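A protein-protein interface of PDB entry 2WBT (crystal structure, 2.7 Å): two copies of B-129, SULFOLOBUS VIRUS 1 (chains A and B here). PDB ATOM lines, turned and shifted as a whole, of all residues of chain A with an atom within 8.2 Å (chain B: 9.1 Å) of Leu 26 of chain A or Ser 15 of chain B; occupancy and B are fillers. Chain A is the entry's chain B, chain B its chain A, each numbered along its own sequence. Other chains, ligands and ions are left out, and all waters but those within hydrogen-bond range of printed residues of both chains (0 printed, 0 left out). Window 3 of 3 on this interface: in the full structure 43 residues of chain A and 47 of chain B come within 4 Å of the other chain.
O of Lys 18 of chain B is in hydrogen-bond range of ND1 of His 23 of chain A.
NZ of Lys 48 of chain B lies within salt-bridge range of OE1 of Glu 28 of chain A.
The side-chain amide oxygen (OD1) of Asn 16 of chain B is in hydrogen-bond range of the backbone NH (N) of Lys 18 of chain B (2.8 Å).
The side-chain hydroxyl of Thr 25 of chain A lies close to the backbone NH of Glu 27 of chain A.
OE1 of Glu 28 of chain A sits at hydrogen-bond distance from N of Thr 25 of chain A (3.1 Å).
The side-chain carboxylate (OE2) of Glu 27 of chain A lies within salt-bridge range of the guanidinium group (NH1) of Arg 31 of chain A (3.9 Å).
A ring nitrogen (ND1) of His 33 of chain A lies within hydrogen-bond range of the backbone carbonyl oxygen of Leu 29 of chain A (3.0 Å).
Among the printed residues, pairs that only touch across the chains: Val 24 of chain A with Lys 48 of chain B (3.7 Å), Val 24 of chain A with Ile 51 of chain B (3.7 Å), Thr 25 of chain A with Lys 48 of chain B (3.8 Å), Leu 26 of chain A with Ser 15 of chain B (3.9 Å), Leu 26 of chain A with Asn 16 of chain B (3.8 Å), Glu 28 of chain A with Ile 51 of chain B (3.8 Å), Leu 29 of chain A with Tyr 13 of chain B (3.8 Å), Leu 29 of chain A with Leu 14 of chain B (3.3 Å), Leu 29 of chain A with Asn 16 of chain B (3.1 Å), Leu 29 of chain A with Gly 19 of chain B (3.5 Å), Leu 29 of chain A with Ile 20 of chain B (3.4 Å), Arg 31 of chain A with Ile 51 of chain B (3.8 Å), Tyr 32 of chain A with Ile 20 of chain B (3.4 Å), His 33 of chain A with Tyr 13 of chain B (3.4 Å) and His 33 of chain A with Leu 14 of chain B (3.9 Å).
Printed residues of chain B within 4 Å of Val 24 of chain A: Lys 48 (3.7 Å) and Ile 51 (3.7 Å).
Thr 25 of chain A touches one residue of chain B.
Of chain B, only Ser 15 (3.9 Å) and Asn 16 (3.8 Å) come within 4 Å of Leu 26 of chain A.
Gln 34 of chain A touches none of the printed residues of chain B.
His 17 of chain B touches none of the printed residues of chain A.
Of the printed residues of chain A, Gly 19 of chain B touches Leu 29.
Of the printed residues of chain A, Lys 48 of chain B touches Val 24, Thr 25 and Glu 28.
Of the printed residues of chain A, Ile 51 of chain B touches Val 24, Glu 28 and Arg 31.
The nearest residue of chain B that does not touch Leu 26 of chain A is His 17 of chain B (4.6 Å).
The nearest residue of chain A that does not touch Ser 15 of chain B is Leu 29 of chain A (4.3 Å).
The nearest printed residue of chain A that does not touch Lys 18 of chain B is Val 24 of chain A (4.3 Å).
Of the 13 printed residues of chain B, 9 touch a printed residue of chain A.
Hydrophobic or aromatic side chains of chain B within 4 Å of the printed part of chain A: Tyr 13, Leu 14, Ile 20 and Ile 51.
Of the 12 printed residues of chain A, 9 touch a printed residue of chain B.
Printed residues of chain A that touch a printed residue of chain B: His 23, Val 24, Thr 25, Leu 26, Glu 28, Leu 29, Arg 31, Tyr 32 and His 33.
No position is printed for both chains.
Of the 17 pairs that touch across the chains among the printed residues, none has its exchanged pair printed and touching as well.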
ATOM      1  N   HIS A  23     -15.895  -0.763  26.347  1.00  0.00           N
ATOM      2  CA  HIS A  23     -15.979   0.199  25.235  1.00  0.00           C
ATOM      3  C   HIS A  23     -16.242   1.637  25.683  1.00  0.00           C
ATOM      4  O   HIS A  23     -17.326   2.184  25.480  1.00  0.00           O
ATOM      5  CB  HIS A  23     -17.031  -0.240  24.209  1.00  0.00           C
ATOM      6  CG  HIS A  23     -16.858  -1.646  23.725  1.00  0.00           C
ATOM      7  ND1 HIS A  23     -15.628  -2.263  23.646  1.00  0.00           N
ATOM      8  CD2 HIS A  23     -17.762  -2.552  23.282  1.00  0.00           C
ATOM      9  CE1 HIS A  23     -15.782  -3.492  23.186  1.00  0.00           C
ATOM     10  NE2 HIS A  23     -17.067  -3.691  22.954  1.00  0.00           N
ATOM     11  N   VAL A  24     -15.216   2.246  26.265  1.00  0.00           N
ATOM     12  CA  VAL A  24     -15.274   3.620  26.762  1.00  0.00           C
ATOM     13  C   VAL A  24     -14.858   4.574  25.640  1.00  0.00           C
ATOM     14  O   VAL A  24     -14.188   4.156  24.693  1.00  0.00           O
ATOM     15  CB  VAL A  24     -14.363   3.779  28.017  1.00  0.00           C
ATOM     16  CG1 VAL A  24     -13.380   4.927  27.865  1.00  0.00           C
ATOM     17  CG2 VAL A  24     -15.207   3.933  29.278  1.00  0.00           C
ATOM     18  N   THR A  25     -15.253   5.843  25.734  1.00  0.00           N
ATOM     19  CA  THR A  25     -14.908   6.813  24.687  1.00  0.00           C
ATOM     20  C   THR A  25     -13.442   7.212  24.771  1.00  0.00           C
ATOM     21  O   THR A  25     -12.792   7.032  25.801  1.00  0.00           O
ATOM     22  CB  THR A  25     -15.764   8.100  24.728  1.00  0.00           C
ATOM     23  OG1 THR A  25     -15.205   9.040  25.660  1.00  0.00           O
ATOM     24  CG2 THR A  25     -17.214   7.794  25.108  1.00  0.00           C
ATOM     25  N   LEU A  26     -12.936   7.771  23.675  1.00  0.00           N
ATOM     26  CA  LEU A  26     -11.523   8.135  23.573  1.00  0.00           C
ATOM     27  C   LEU A  26     -11.099   9.141  24.643  1.00  0.00           C
ATOM     28  O   LEU A  26      -9.982   9.068  25.157  1.00  0.00           O
ATOM     29  CB  LEU A  26     -11.205   8.687  22.181  1.00  0.00           C
ATOM     30  CG  LEU A  26     -11.145   7.664  21.042  1.00  0.00           C
ATOM     31  CD1 LEU A  26     -10.918   8.367  19.712  1.00  0.00           C
ATOM     32  CD2 LEU A  26     -10.058   6.626  21.290  1.00  0.00           C
ATOM     33  N   GLU A  27     -11.986  10.082  24.965  1.00  0.00           N
ATOM     34  CA  GLU A  27     -11.749  11.013  26.070  1.00  0.00           C
ATOM     35  C   GLU A  27     -11.635  10.238  27.383  1.00  0.00           C
ATOM     36  O   GLU A  27     -10.631  10.340  28.082  1.00  0.00           O
ATOM     37  CB  GLU A  27     -12.861  12.074  26.142  1.00  0.00           C
ATOM     38  CG  GLU A  27     -13.058  12.766  27.504  1.00  0.00           C
ATOM     39  CD  GLU A  27     -11.892  13.652  27.926  1.00  0.00           C
ATOM     40  OE1 GLU A  27     -10.727  13.292  27.675  1.00  0.00           O
ATOM     41  OE2 GLU A  27     -12.149  14.717  28.528  1.00  0.00           O
ATOM     42  N   GLU A  28     -12.657   9.445  27.690  1.00  0.00           N
ATOM     43  CA  GLU A  28     -12.693   8.646  28.920  1.00  0.00           C
ATOM     44  C   GLU A  28     -11.517   7.667  29.042  1.00  0.00           C
ATOM     45  O   GLU A  28     -11.103   7.327  30.150  1.00  0.00           O
ATOM     46  CB  GLU A  28     -14.017   7.883  29.012  1.00  0.00           C
ATOM     47  CG  GLU A  28     -15.229   8.772  29.278  1.00  0.00           C
ATOM     48  CD  GLU A  28     -16.550   8.129  28.876  1.00  0.00           C
ATOM     49  OE1 GLU A  28     -16.539   7.043  28.256  1.00  0.00           O
ATOM     50  OE2 GLU A  28     -17.608   8.717  29.179  1.00  0.00           O
ATOM     51  N   LEU A  29     -10.987   7.220  27.903  1.00  0.00           N
ATOM     52  CA  LEU A  29      -9.842   6.308  27.877  1.00  0.00           C
ATOM     53  C   LEU A  29      -8.536   7.000  28.282  1.00  0.00           C
ATOM     54  O   LEU A  29      -7.741   6.428  29.029  1.00  0.00           O
ATOM     55  CB  LEU A  29      -9.690   5.673  26.489  1.00  0.00           C
ATOM     56  CG  LEU A  29      -8.611   4.593  26.342  1.00  0.00           C
ATOM     57  CD1 LEU A  29      -8.897   3.404  27.245  1.00  0.00           C
ATOM     58  CD2 LEU A  29      -8.504   4.149  24.893  1.00  0.00           C
ATOM     59  N   LYS A  30      -8.306   8.212  27.781  1.00  0.00           N
ATOM     60  CA  LYS A  30      -7.127   8.992  28.188  1.00  0.00           C
ATOM     61  C   LYS A  30      -7.313   9.570  29.595  1.00  0.00           C
ATOM     62  O   LYS A  30      -6.342   9.759  30.327  1.00  0.00           O
ATOM     63  CB  LYS A  30      -6.787  10.093  27.170  1.00  0.00           C
ATOM     64  CG  LYS A  30      -7.764  11.259  27.082  1.00  0.00           C
ATOM     65  CD  LYS A  30      -7.204  12.354  26.180  1.00  0.00           C
ATOM     66  CE  LYS A  30      -8.106  13.574  26.129  1.00  0.00           C
ATOM     67  NZ  LYS A  30      -7.535  14.655  25.277  1.00  0.00           N
ATOM     68  N   ARG A  31      -8.564   9.851  29.954  1.00  0.00           N
ATOM     69  CA  ARG A  31      -8.927  10.214  31.327  1.00  0.00           C
ATOM     70  C   ARG A  31      -8.621   9.063  32.281  1.00  0.00           C
ATOM     71  O   ARG A  31      -8.093   9.271  33.374  1.00  0.00           O
ATOM     72  CB  ARG A  31     -10.417  10.545  31.418  1.00  0.00           C
ATOM     73  CG  ARG A  31     -10.832  11.815  30.686  1.00  0.00           C
ATOM     74  CD  ARG A  31     -10.501  13.068  31.471  1.00  0.00           C
ATOM     75  NE  ARG A  31     -11.100  13.048  32.803  1.00  0.00           N
ATOM     76  CZ  ARG A  31     -12.386  13.269  33.068  1.00  0.00           C
ATOM     77  NH1 ARG A  31     -13.255  13.539  32.096  1.00  0.00           N
ATOM     78  NH2 ARG A  31     -12.813  13.220  34.325  1.00  0.00           N
ATOM     79  N   TYR A  32      -8.972   7.853  31.852  1.00  0.00           N
ATOM     80  CA  TYR A  32      -8.735   6.635  32.630  1.00  0.00           C
ATOM     81  C   TYR A  32      -7.256   6.441  32.956  1.00  0.00           C
ATOM     82  O   TYR A  32      -6.894   6.208  34.109  1.00  0.00           O
ATOM     83  CB  TYR A  32      -9.254   5.407  31.875  1.00  0.00           C
ATOM     84  CG  TYR A  32      -8.865   4.090  32.510  1.00  0.00           C
ATOM     85  CD1 TYR A  32      -7.839   3.311  31.978  1.00  0.00           C
ATOM     86  CD2 TYR A  32      -9.518   3.628  33.649  1.00  0.00           C
ATOM     87  CE1 TYR A  32      -7.477   2.104  32.561  1.00  0.00           C
ATOM     88  CE2 TYR A  32      -9.164   2.422  34.239  1.00  0.00           C
ATOM     89  CZ  TYR A  32      -8.145   1.664  33.690  1.00  0.00           C
ATOM     90  OH  TYR A  32      -7.791   0.470  34.273  1.00  0.00           O
ATOM     91  N   HIS A  33      -6.411   6.540  31.935  1.00  0.00           N
ATOM     92  CA  HIS A  33      -4.968   6.317  32.096  1.00  0.00           C
ATOM     93  C   HIS A  33      -4.231   7.457  32.811  1.00  0.00           C
ATOM     94  O   HIS A  33      -3.031   7.352  33.069  1.00  0.00           O
ATOM     95  CB  HIS A  33      -4.322   6.023  30.738  1.00  0.00           C
ATOM     96  CG  HIS A  33      -4.620   4.651  30.222  1.00  0.00           C
ATOM     97  ND1 HIS A  33      -5.494   4.418  29.182  1.00  0.00           N
ATOM     98  CD2 HIS A  33      -4.174   3.435  30.617  1.00  0.00           C
ATOM     99  CE1 HIS A  33      -5.564   3.118  28.952  1.00  0.00           C
ATOM    100  NE2 HIS A  33      -4.774   2.500  29.809  1.00  0.00           N
ATOM    101  N   GLN A  34      -4.945   8.537  33.125  1.00  0.00           N
ATOM    102  CA  GLN A  34      -4.411   9.603  33.976  1.00  0.00           C
ATOM    103  C   GLN A  34      -4.722   9.367  35.455  1.00  0.00           C
ATOM    104  O   GLN A  34      -4.227  10.096  36.317  1.00  0.00           O
ATOM    105  CB  GLN A  34      -4.948  10.960  33.522  1.00  0.00           C
ATOM    106  CG  GLN A  34      -4.284  11.457  32.247  1.00  0.00           C
ATOM    107  CD  GLN A  34      -5.022  12.615  31.606  1.00  0.00           C
ATOM    108  OE1 GLN A  34      -6.237  12.568  31.418  1.00  0.00           O
ATOM    109  NE2 GLN A  34      -4.284  13.662  31.255  1.00  0.00           N
ATOM    110  N   SER B  10       4.460  -0.910  23.828  1.00  0.00           N
ATOM    111  CA  SER B  10       3.596  -0.271  22.839  1.00  0.00           C
ATOM    112  C   SER B  10       2.689   0.742  23.532  1.00  0.00           C
ATOM    113  O   SER B  10       2.240   0.509  24.655  1.00  0.00           O
ATOM    114  CB  SER B  10       2.747  -1.318  22.114  1.00  0.00           C
ATOM    115  OG  SER B  10       1.876  -0.713  21.177  1.00  0.00           O
ATOM    116  N   LYS B  11       2.430   1.863  22.862  1.00  0.00           N
ATOM    117  CA  LYS B  11       1.621   2.946  23.434  1.00  0.00           C
ATOM    118  C   LYS B  11       0.278   3.159  22.722  1.00  0.00           C
ATOM    119  O   LYS B  11      -0.367   4.192  22.912  1.00  0.00           O
ATOM    120  CB  LYS B  11       2.428   4.252  23.458  1.00  0.00           C
ATOM    121  CG  LYS B  11       3.260   4.433  24.723  1.00  0.00           C
ATOM    122  CD  LYS B  11       4.133   5.682  24.669  1.00  0.00           C
ATOM    123  CE  LYS B  11       5.257   5.546  23.654  1.00  0.00           C
ATOM    124  NZ  LYS B  11       6.232   6.667  23.748  1.00  0.00           N
ATOM    125  N   LYS B  12      -0.154   2.185  21.922  1.00  0.00           N
ATOM    126  CA  LYS B  12      -1.466   2.269  21.259  1.00  0.00           C
ATOM    127  C   LYS B  12      -2.619   1.820  22.163  1.00  0.00           C
ATOM    128  O   LYS B  12      -3.786   1.981  21.801  1.00  0.00           O
ATOM    129  CB  LYS B  12      -1.495   1.497  19.933  1.00  0.00           C
ATOM    130  CG  LYS B  12      -1.057   0.046  20.011  1.00  0.00           C
ATOM    131  CD  LYS B  12      -1.666  -0.782  18.888  1.00  0.00           C
ATOM    132  CE  LYS B  12      -0.919  -2.094  18.692  1.00  0.00           C
ATOM    133  NZ  LYS B  12      -0.690  -2.821  19.974  1.00  0.00           N
ATOM    134  N   TYR B  13      -2.299   1.254  23.327  1.00  0.00           N
ATOM    135  CA  TYR B  13      -3.309   1.007  24.364  1.00  0.00           C
ATOM    136  C   TYR B  13      -3.995   2.322  24.763  1.00  0.00           C
ATOM    137  O   TYR B  13      -5.166   2.328  25.146  1.00  0.00           O
ATOM    138  CB  TYR B  13      -2.684   0.337  25.597  1.00  0.00           C
ATOM    139  CG  TYR B  13      -1.809   1.253  26.426  1.00  0.00           C
ATOM    140  CD1 TYR B  13      -2.354   2.062  27.421  1.00  0.00           C
ATOM    141  CD2 TYR B  13      -0.437   1.313  26.213  1.00  0.00           C
ATOM    142  CE1 TYR B  13      -1.556   2.907  28.178  1.00  0.00           C
ATOM    143  CE2 TYR B  13       0.372   2.153  26.967  1.00  0.00           C
ATOM    144  CZ  TYR B  13      -0.194   2.948  27.948  1.00  0.00           C
ATOM    145  OH  TYR B  13       0.603   3.783  28.697  1.00  0.00           O
ATOM    146  N   LEU B  14      -3.248   3.423  24.676  1.00  0.00           N
ATOM    147  CA  LEU B  14      -3.763   4.763  24.985  1.00  0.00           C
ATOM    148  C   LEU B  14      -4.874   5.235  24.039  1.00  0.00           C
ATOM    149  O   LEU B  14      -5.772   5.965  24.460  1.00  0.00           O
ATOM    150  CB  LEU B  14      -2.625   5.795  24.961  1.00  0.00           C
ATOM    151  CG  LEU B  14      -1.611   5.768  26.107  1.00  0.00           C
ATOM    152  CD1 LEU B  14      -0.491   6.763  25.845  1.00  0.00           C
ATOM    153  CD2 LEU B  14      -2.284   6.061  27.441  1.00  0.00           C
ATOM    154  N   SER B  15      -4.809   4.820  22.775  1.00  0.00           N
ATOM    155  CA  SER B  15      -5.707   5.336  21.732  1.00  0.00           C
ATOM    156  C   SER B  15      -6.572   4.260  21.067  1.00  0.00           C
ATOM    157  O   SER B  15      -7.120   4.485  19.985  1.00  0.00           O
ATOM    158  CB  SER B  15      -4.888   6.057  20.659  1.00  0.00           C
ATOM    159  OG  SER B  15      -5.725   6.786  19.777  1.00  0.00           O
ATOM    160  N   ASN B  16      -6.694   3.100  21.709  1.00  0.00           N
ATOM    161  CA  ASN B  16      -7.510   2.008  21.174  1.00  0.00           C
ATOM    162  C   ASN B  16      -8.994   2.377  21.191  1.00  0.00           C
ATOM    163  O   ASN B  16      -9.489   2.956  22.159  1.00  0.00           O
ATOM    164  CB  ASN B  16      -7.269   0.715  21.963  1.00  0.00           C
ATOM    165  CG  ASN B  16      -7.786  -0.521  21.242  1.00  0.00           C
ATOM    166  OD1 ASN B  16      -8.886  -0.522  20.688  1.00  0.00           O
ATOM    167  ND2 ASN B  16      -6.992  -1.586  21.253  1.00  0.00           N
ATOM    168  N   HIS B  17      -9.693   2.031  20.113  1.00  0.00           N
ATOM    169  CA  HIS B  17     -11.103   2.397  19.939  1.00  0.00           C
ATOM    170  C   HIS B  17     -12.029   1.466  20.722  1.00  0.00           C
ATOM    171  O   HIS B  17     -13.105   1.877  21.162  1.00  0.00           O
ATOM    172  CB  HIS B  17     -11.471   2.384  18.455  1.00  0.00           C
ATOM    173  CG  HIS B  17     -10.640   3.312  17.623  1.00  0.00           C
ATOM    174  ND1 HIS B  17      -9.331   3.038  17.286  1.00  0.00           N
ATOM    175  CD2 HIS B  17     -10.929   4.511  17.063  1.00  0.00           C
ATOM    176  CE1 HIS B  17      -8.851   4.027  16.556  1.00  0.00           C
ATOM    177  NE2 HIS B  17      -9.800   4.933  16.405  1.00  0.00           N
ATOM    178  N   LYS B  18     -11.605   0.214  20.885  1.00  0.00           N
ATOM    179  CA  LYS B  18     -12.301  -0.749  21.747  1.00  0.00           C
ATOM    180  C   LYS B  18     -12.301  -0.309  23.213  1.00  0.00           C
ATOM    181  O   LYS B  18     -13.131  -0.764  23.997  1.00  0.00           O
ATOM    182  CB  LYS B  18     -11.662  -2.136  21.637  1.00  0.00           C
ATOM    183  CG  LYS B  18     -12.049  -2.918  20.394  1.00  0.00           C
ATOM    184  CD  LYS B  18     -11.061  -4.049  20.138  1.00  0.00           C
ATOM    185  CE  LYS B  18     -11.651  -5.128  19.245  1.00  0.00           C
ATOM    186  NZ  LYS B  18     -10.745  -6.304  19.122  1.00  0.00           N
ATOM    187  N   GLY B  19     -11.344   0.542  23.580  1.00  0.00           N
ATOM    188  CA  GLY B  19     -11.342   1.201  24.886  1.00  0.00           C
ATOM    189  C   GLY B  19     -10.404   0.579  25.904  1.00  0.00           C
ATOM    190  O   GLY B  19      -9.304   0.139  25.567  1.00  0.00           O
ATOM    191  N   ILE B  20     -10.853   0.550  27.157  1.00  0.00           N
ATOM    192  CA  ILE B  20     -10.038   0.102  28.287  1.00  0.00           C
ATOM    193  C   ILE B  20      -9.841  -1.411  28.288  1.00  0.00           C
ATOM    194  O   ILE B  20     -10.811  -2.164  28.373  1.00  0.00           O
ATOM    195  CB  ILE B  20     -10.690   0.502  29.632  1.00  0.00           C
ATOM    196  CG1 ILE B  20     -10.618   2.015  29.838  1.00  0.00           C
ATOM    197  CG2 ILE B  20     -10.001  -0.201  30.796  1.00  0.00           C
ATOM    198  CD1 ILE B  20     -11.457   2.509  30.997  1.00  0.00           C
ATOM    199  N   LYS B  48     -17.765   4.104  33.401  1.00  0.00           N
ATOM    200  CA  LYS B  48     -17.833   5.488  32.925  1.00  0.00           C
ATOM    201  C   LYS B  48     -18.082   6.465  34.078  1.00  0.00           C
ATOM    202  O   LYS B  48     -17.444   7.515  34.155  1.00  0.00           O
ATOM    203  CB  LYS B  48     -18.922   5.647  31.860  1.00  0.00           C
ATOM    204  CG  LYS B  48     -18.541   5.088  30.498  1.00  0.00           C
ATOM    205  CD  LYS B  48     -19.560   5.468  29.434  1.00  0.00           C
ATOM    206  CE  LYS B  48     -19.161   4.947  28.063  1.00  0.00           C
ATOM    207  NZ  LYS B  48     -19.826   5.702  26.965  1.00  0.00           N
ATOM    208  N   ILE B  51     -14.953   6.697  36.165  1.00  0.00           N
ATOM    209  CA  ILE B  51     -13.981   7.540  35.462  1.00  0.00           C
ATOM    210  C   ILE B  51     -14.245   9.036  35.682  1.00  0.00           C
ATOM    211  O   ILE B  51     -13.306   9.809  35.883  1.00  0.00           O
ATOM    212  CB  ILE B  51     -13.961   7.232  33.942  1.00  0.00           C
ATOM    213  CG1 ILE B  51     -13.284   5.886  33.679  1.00  0.00           C
ATOM    214  CG2 ILE B  51     -13.224   8.322  33.174  1.00  0.00           C
ATOM    215  CD1 ILE B  51     -13.495   5.362  32.276  1.00  0.00           C
